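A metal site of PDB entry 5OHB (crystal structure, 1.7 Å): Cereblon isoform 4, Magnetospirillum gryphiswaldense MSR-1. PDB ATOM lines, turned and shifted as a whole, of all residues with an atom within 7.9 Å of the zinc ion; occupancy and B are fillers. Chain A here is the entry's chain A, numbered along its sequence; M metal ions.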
ATOM      1  N   ARG A  24      20.827  -1.806 -33.746  1.00  0.00           N
ATOM      2  CA  ARG A  24      20.880  -3.223 -33.503  1.00  0.00           C
ATOM      3  C   ARG A  24      20.490  -3.534 -32.081  1.00  0.00           C
ATOM      4  O   ARG A  24      20.619  -2.678 -31.196  1.00  0.00           O
ATOM      5  CB  ARG A  24      22.312  -3.773 -33.768  1.00  0.00           C
ATOM      6  CG  ARG A  24      22.656  -3.799 -35.231  1.00  0.00           C
ATOM      7  CD  ARG A  24      24.052  -4.346 -35.590  1.00  0.00           C
ATOM      8  NE  ARG A  24      24.316  -4.327 -37.004  1.00  0.00           N
ATOM      9  CZ  ARG A  24      23.757  -5.137 -37.886  1.00  0.00           C
ATOM     10  NH1 ARG A  24      23.066  -6.176 -37.447  1.00  0.00           N
ATOM     11  NH2 ARG A  24      23.984  -4.991 -39.191  1.00  0.00           N
ATOM     12  N   CYS A  25      20.044  -4.773 -31.833  1.00  0.00           N
ATOM     13  CA  CYS A  25      19.838  -5.212 -30.448  1.00  0.00           C
ATOM     14  C   CYS A  25      21.168  -5.147 -29.673  1.00  0.00           C
ATOM     15  O   CYS A  25      22.166  -5.662 -30.141  1.00  0.00           O
ATOM     16  CB  CYS A  25      19.340  -6.650 -30.435  1.00  0.00           C
ATOM     17  SG  CYS A  25      19.155  -7.334 -28.746  1.00  0.00           S
ATOM     18  N   ARG A  26      21.198  -4.475 -28.536  1.00  0.00           N
ATOM     19  CA  ARG A  26      22.405  -4.336 -27.768  1.00  0.00           C
ATOM     20  C   ARG A  26      22.911  -5.678 -27.238  1.00  0.00           C
ATOM     21  O   ARG A  26      24.109  -5.795 -26.958  1.00  0.00           O
ATOM     22  CB  ARG A  26      22.129  -3.384 -26.589  1.00  0.00           C
ATOM     23  CG  ARG A  26      23.200  -3.123 -25.663  1.00  0.00           C
ATOM     24  CD  ARG A  26      22.732  -2.153 -24.590  1.00  0.00           C
ATOM     25  NE  ARG A  26      23.744  -2.010 -23.603  1.00  0.00           N
ATOM     26  CZ  ARG A  26      23.685  -1.226 -22.546  1.00  0.00           C
ATOM     27  NH1 ARG A  26      22.651  -0.392 -22.332  1.00  0.00           N
ATOM     28  NH2 ARG A  26      24.691  -1.262 -21.733  1.00  0.00           N
ATOM     29  N   GLN A  27      21.993  -6.598 -26.985  1.00  0.00           N
ATOM     30  CA  GLN A  27      22.382  -7.867 -26.387  1.00  0.00           C
ATOM     31  C   GLN A  27      22.959  -8.870 -27.377  1.00  0.00           C
ATOM     32  O   GLN A  27      23.719  -9.738 -26.945  1.00  0.00           O
ATOM     33  CB  GLN A  27      21.171  -8.433 -25.665  1.00  0.00           C
ATOM     34  CG  GLN A  27      20.779  -7.545 -24.515  1.00  0.00           C
ATOM     35  CD  GLN A  27      21.947  -7.240 -23.555  1.00  0.00           C
ATOM     36  OE1 GLN A  27      22.275  -6.074 -23.257  1.00  0.00           O
ATOM     37  NE2 GLN A  27      22.576  -8.296 -23.065  1.00  0.00           N
ATOM     38  N   CYS A  28      22.658  -8.750 -28.662  1.00  0.00           N
ATOM     39  CA  CYS A  28      23.089  -9.800 -29.590  1.00  0.00           C
ATOM     40  C   CYS A  28      23.496  -9.286 -30.947  1.00  0.00           C
ATOM     41  O   CYS A  28      24.148 -10.022 -31.689  1.00  0.00           O
ATOM     42  CB  CYS A  28      22.020 -10.868 -29.711  1.00  0.00           C
ATOM     43  SG  CYS A  28      20.585 -10.318 -30.693  1.00  0.00           S
ATOM     44  N   GLY A  29      23.120  -8.054 -31.348  1.00  0.00           N
ATOM     45  CA  GLY A  29      23.433  -7.624 -32.680  1.00  0.00           C
ATOM     46  C   GLY A  29      22.424  -7.709 -33.790  1.00  0.00           C
ATOM     47  O   GLY A  29      22.656  -7.169 -34.878  1.00  0.00           O
ATOM     48  N   GLN A  30      21.302  -8.363 -33.538  1.00  0.00           N
ATOM     49  CA  GLN A  30      20.205  -8.403 -34.455  1.00  0.00           C
ATOM     50  C   GLN A  30      19.871  -7.006 -35.035  1.00  0.00           C
ATOM     51  O   GLN A  30      19.752  -6.061 -34.255  1.00  0.00           O
ATOM     52  CB  GLN A  30      18.988  -8.904 -33.688  1.00  0.00           C
ATOM     53  CG  GLN A  30      17.684  -8.952 -34.449  1.00  0.00           C
ATOM     54  CD  GLN A  30      17.637 -10.142 -35.403  1.00  0.00           C
ATOM     55  OE1 GLN A  30      18.640 -10.485 -36.033  1.00  0.00           O
ATOM     56  NE2 GLN A  30      16.490 -10.766 -35.517  1.00  0.00           N
ATOM     57  N   THR A  31      19.705  -6.906 -36.332  1.00  0.00           N
ATOM     58  CA  THR A  31      19.311  -5.654 -37.028  1.00  0.00           C
ATOM     59  C   THR A  31      17.840  -5.369 -36.666  1.00  0.00           C
ATOM     60  O   THR A  31      17.009  -6.254 -36.822  1.00  0.00           O
ATOM     61  CB  THR A  31      19.459  -5.752 -38.532  1.00  0.00           C
ATOM     62  OG1 THR A  31      20.756  -6.264 -38.836  1.00  0.00           O
ATOM     63  CG2 THR A  31      19.382  -4.412 -39.091  1.00  0.00           C
ATOM     64  N   ILE A  32      17.566  -4.164 -36.147  1.00  0.00           N
ATOM     65  CA  ILE A  32      16.247  -3.830 -35.643  1.00  0.00           C
ATOM     66  C   ILE A  32      15.621  -2.619 -36.383  1.00  0.00           C
ATOM     67  O   ILE A  32      14.505  -2.695 -36.885  1.00  0.00           O
ATOM     68  CB  ILE A  32      16.217  -3.521 -34.144  1.00  0.00           C
ATOM     69  CG1 ILE A  32      16.718  -4.683 -33.304  1.00  0.00           C
ATOM     70  CG2 ILE A  32      14.775  -3.153 -33.728  1.00  0.00           C
ATOM     71  CD1 ILE A  32      15.908  -5.948 -33.415  1.00  0.00           C
ATOM     72  N   GLY A  67      13.296  -7.671 -37.424  1.00  0.00           N
ATOM     73  CA  GLY A  67      14.065  -8.572 -36.533  1.00  0.00           C
ATOM     74  C   GLY A  67      13.497  -8.745 -35.140  1.00  0.00           C
ATOM     75  O   GLY A  67      14.183  -9.260 -34.259  1.00  0.00           O
ATOM     76  N   LEU A  90       9.806  -8.543 -28.717  1.00  0.00           N
ATOM     77  CA  LEU A  90      11.093  -9.093 -28.307  1.00  0.00           C
ATOM     78  C   LEU A  90      12.064  -9.038 -29.475  1.00  0.00           C
ATOM     79  O   LEU A  90      11.663  -9.093 -30.647  1.00  0.00           O
ATOM     80  CB  LEU A  90      10.978 -10.563 -27.810  1.00  0.00           C
ATOM     81  CG  LEU A  90       9.984 -10.790 -26.636  1.00  0.00           C
ATOM     82  CD1 LEU A  90      10.050 -12.269 -26.310  1.00  0.00           C
ATOM     83  CD2 LEU A  90      10.265  -9.845 -25.462  1.00  0.00           C
ATOM     84  N   CYS A  91      13.361  -8.927 -29.168  1.00  0.00           N
ATOM     85  CA  CYS A  91      14.344  -9.257 -30.179  1.00  0.00           C
ATOM     86  C   CYS A  91      14.014 -10.695 -30.699  1.00  0.00           C
ATOM     87  O   CYS A  91      13.934 -11.668 -29.928  1.00  0.00           O
ATOM     88  CB  CYS A  91      15.765  -9.248 -29.589  1.00  0.00           C
ATOM     89  SG  CYS A  91      17.044  -9.707 -30.790  1.00  0.00           S
ATOM     90  N   GLY A  92      13.921 -10.844 -32.029  1.00  0.00           N
ATOM     91  CA  GLY A  92      13.650 -12.117 -32.657  1.00  0.00           C
ATOM     92  C   GLY A  92      14.752 -13.121 -32.520  1.00  0.00           C
ATOM     93  O   GLY A  92      14.534 -14.334 -32.705  1.00  0.00           O
ATOM     94  N   GLN A  93      15.956 -12.637 -32.276  1.00  0.00           N
ATOM     95  CA  GLN A  93      17.120 -13.484 -32.185  1.00  0.00           C
ATOM     96  C   GLN A  93      17.320 -13.950 -30.725  1.00  0.00           C
ATOM     97  O   GLN A  93      17.274 -15.126 -30.463  1.00  0.00           O
ATOM     98  CB  GLN A  93      18.328 -12.771 -32.733  1.00  0.00           C
ATOM     99  CG  GLN A  93      19.605 -13.589 -32.791  1.00  0.00           C
ATOM    100  CD  GLN A  93      20.609 -13.005 -33.766  1.00  0.00           C
ATOM    101  OE1 GLN A  93      20.690 -13.480 -34.875  1.00  0.00           O
ATOM    102  NE2 GLN A  93      21.373 -12.002 -33.360  1.00  0.00           N
ATOM    103  N   CYS A  94      17.459 -13.022 -29.779  1.00  0.00           N
ATOM    104  CA  CYS A  94      17.847 -13.365 -28.431  1.00  0.00           C
ATOM    105  C   CYS A  94      16.724 -13.319 -27.395  1.00  0.00           C
ATOM    106  O   CYS A  94      16.924 -13.806 -26.296  1.00  0.00           O
ATOM    107  CB  CYS A  94      19.028 -12.508 -27.961  1.00  0.00           C
ATOM    108  SG  CYS A  94      18.565 -10.816 -27.438  1.00  0.00           S
ATOM    109  N   GLY A  95      15.589 -12.739 -27.742  1.00  0.00           N
ATOM    110  CA  GLY A  95      14.437 -12.676 -26.833  1.00  0.00           C
ATOM    111  C   GLY A  95      14.450 -11.528 -25.860  1.00  0.00           C
ATOM    112  O   GLY A  95      13.515 -11.423 -25.052  1.00  0.00           O
ATOM    113  N   SER A  96      15.428 -10.653 -25.937  1.00  0.00           N
ATOM    114  CA  SER A  96      15.465  -9.417 -25.167  1.00  0.00           C
ATOM    115  C   SER A  96      14.248  -8.537 -25.417  1.00  0.00           C
ATOM    116  O   SER A  96      13.795  -8.386 -26.540  1.00  0.00           O
ATOM    117  CB  SER A  96      16.729  -8.611 -25.508  1.00  0.00           C
ATOM    118  OG  SER A  96      16.763  -7.366 -24.800  1.00  0.00           O
ATOM    119  N   HIS A  97      13.645  -8.012 -24.323  1.00  0.00           N
ATOM    120  CA  HIS A  97      12.505  -7.121 -24.515  1.00  0.00           C
ATOM    121  C   HIS A  97      12.944  -5.786 -25.018  1.00  0.00           C
ATOM    122  O   HIS A  97      13.559  -5.029 -24.274  1.00  0.00           O
ATOM    123  CB  HIS A  97      11.759  -6.969 -23.189  1.00  0.00           C
ATOM    124  CG  HIS A  97      10.588  -6.089 -23.295  1.00  0.00           C
ATOM    125  ND1 HIS A  97      10.090  -5.382 -22.216  1.00  0.00           N
ATOM    126  CD2 HIS A  97       9.815  -5.759 -24.363  1.00  0.00           C
ATOM    127  CE1 HIS A  97       9.048  -4.676 -22.614  1.00  0.00           C
ATOM    128  NE2 HIS A  97       8.864  -4.880 -23.905  1.00  0.00           N
ATOM    129  N   LEU A  98      12.674  -5.467 -26.286  1.00  0.00           N
ATOM    130  CA  LEU A  98      13.079  -4.271 -26.948  1.00  0.00           C
ATOM    131  C   LEU A  98      12.049  -3.159 -27.000  1.00  0.00           C
ATOM    132  O   LEU A  98      12.400  -2.010 -27.169  1.00  0.00           O
ATOM    133  CB  LEU A  98      13.595  -4.550 -28.352  1.00  0.00           C
ATOM    134  CG  LEU A  98      14.831  -5.485 -28.443  1.00  0.00           C
ATOM    135  CD1 LEU A  98      15.305  -5.597 -29.883  1.00  0.00           C
ATOM    136  CD2 LEU A  98      15.943  -5.051 -27.529  1.00  0.00           C
ATOM    137  N   ARG A 118      18.200  -0.162 -24.999  1.00  0.00           N
ATOM    138  CA  ARG A 118      18.345  -1.561 -25.343  1.00  0.00           C
ATOM    139  C   ARG A 118      18.857  -1.755 -26.777  1.00  0.00           C
ATOM    140  O   ARG A 118      18.855  -2.891 -27.254  1.00  0.00           O
ATOM    141  CB  ARG A 118      17.009  -2.278 -25.124  1.00  0.00           C
ATOM    142  CG  ARG A 118      16.628  -2.130 -23.661  1.00  0.00           C
ATOM    143  CD  ARG A 118      15.651  -3.158 -23.129  1.00  0.00           C
ATOM    144  NE  ARG A 118      15.315  -2.747 -21.745  1.00  0.00           N
ATOM    145  CZ  ARG A 118      14.313  -3.255 -21.031  1.00  0.00           C
ATOM    146  NH1 ARG A 118      13.576  -4.265 -21.535  1.00  0.00           N
ATOM    147  NH2 ARG A 118      14.069  -2.765 -19.791  1.00  0.00           N
HETATM  148 ZN    ZN M   1      18.879  -9.530 -29.342  1.00  0.00          ZN
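SG of Cys 25 lies close to N of Gln 27, 3.4 Å away.
SG of Cys 28 sits close to N of Gln 30 (3.5 Å).
N of Cys 91 is in hydrogen-bond range of O of Ser 96, at 2.7 Å.
The backbone NH (N) of Cys 25 sits at hydrogen-bond distance from the backbone carbonyl oxygen (O) of Gln 30, 2.8 Å away.
The side-chain sulfur of Cys 28 sits close to the side-chain amide nitrogen of Gln 93, at 3.3 Å.
SG of Cys 94 sits close to N of Ser 96, 3.5 Å away.
SG of Cys 91 sits close to N of Gln 93, at 3.5 Å.
Of the 20 residues printed, 4 come within 4 Å of the zinc ion.
The nearest printed residue that does not touch the zinc ion is Gln 30 (4.4 Å).
The zinc ion is bound by the side-chain sulfur of Cys 25, the side-chain sulfur of Cys 28, the side-chain sulfur of Cys 94 and the side-chain sulfur of Cys 91.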
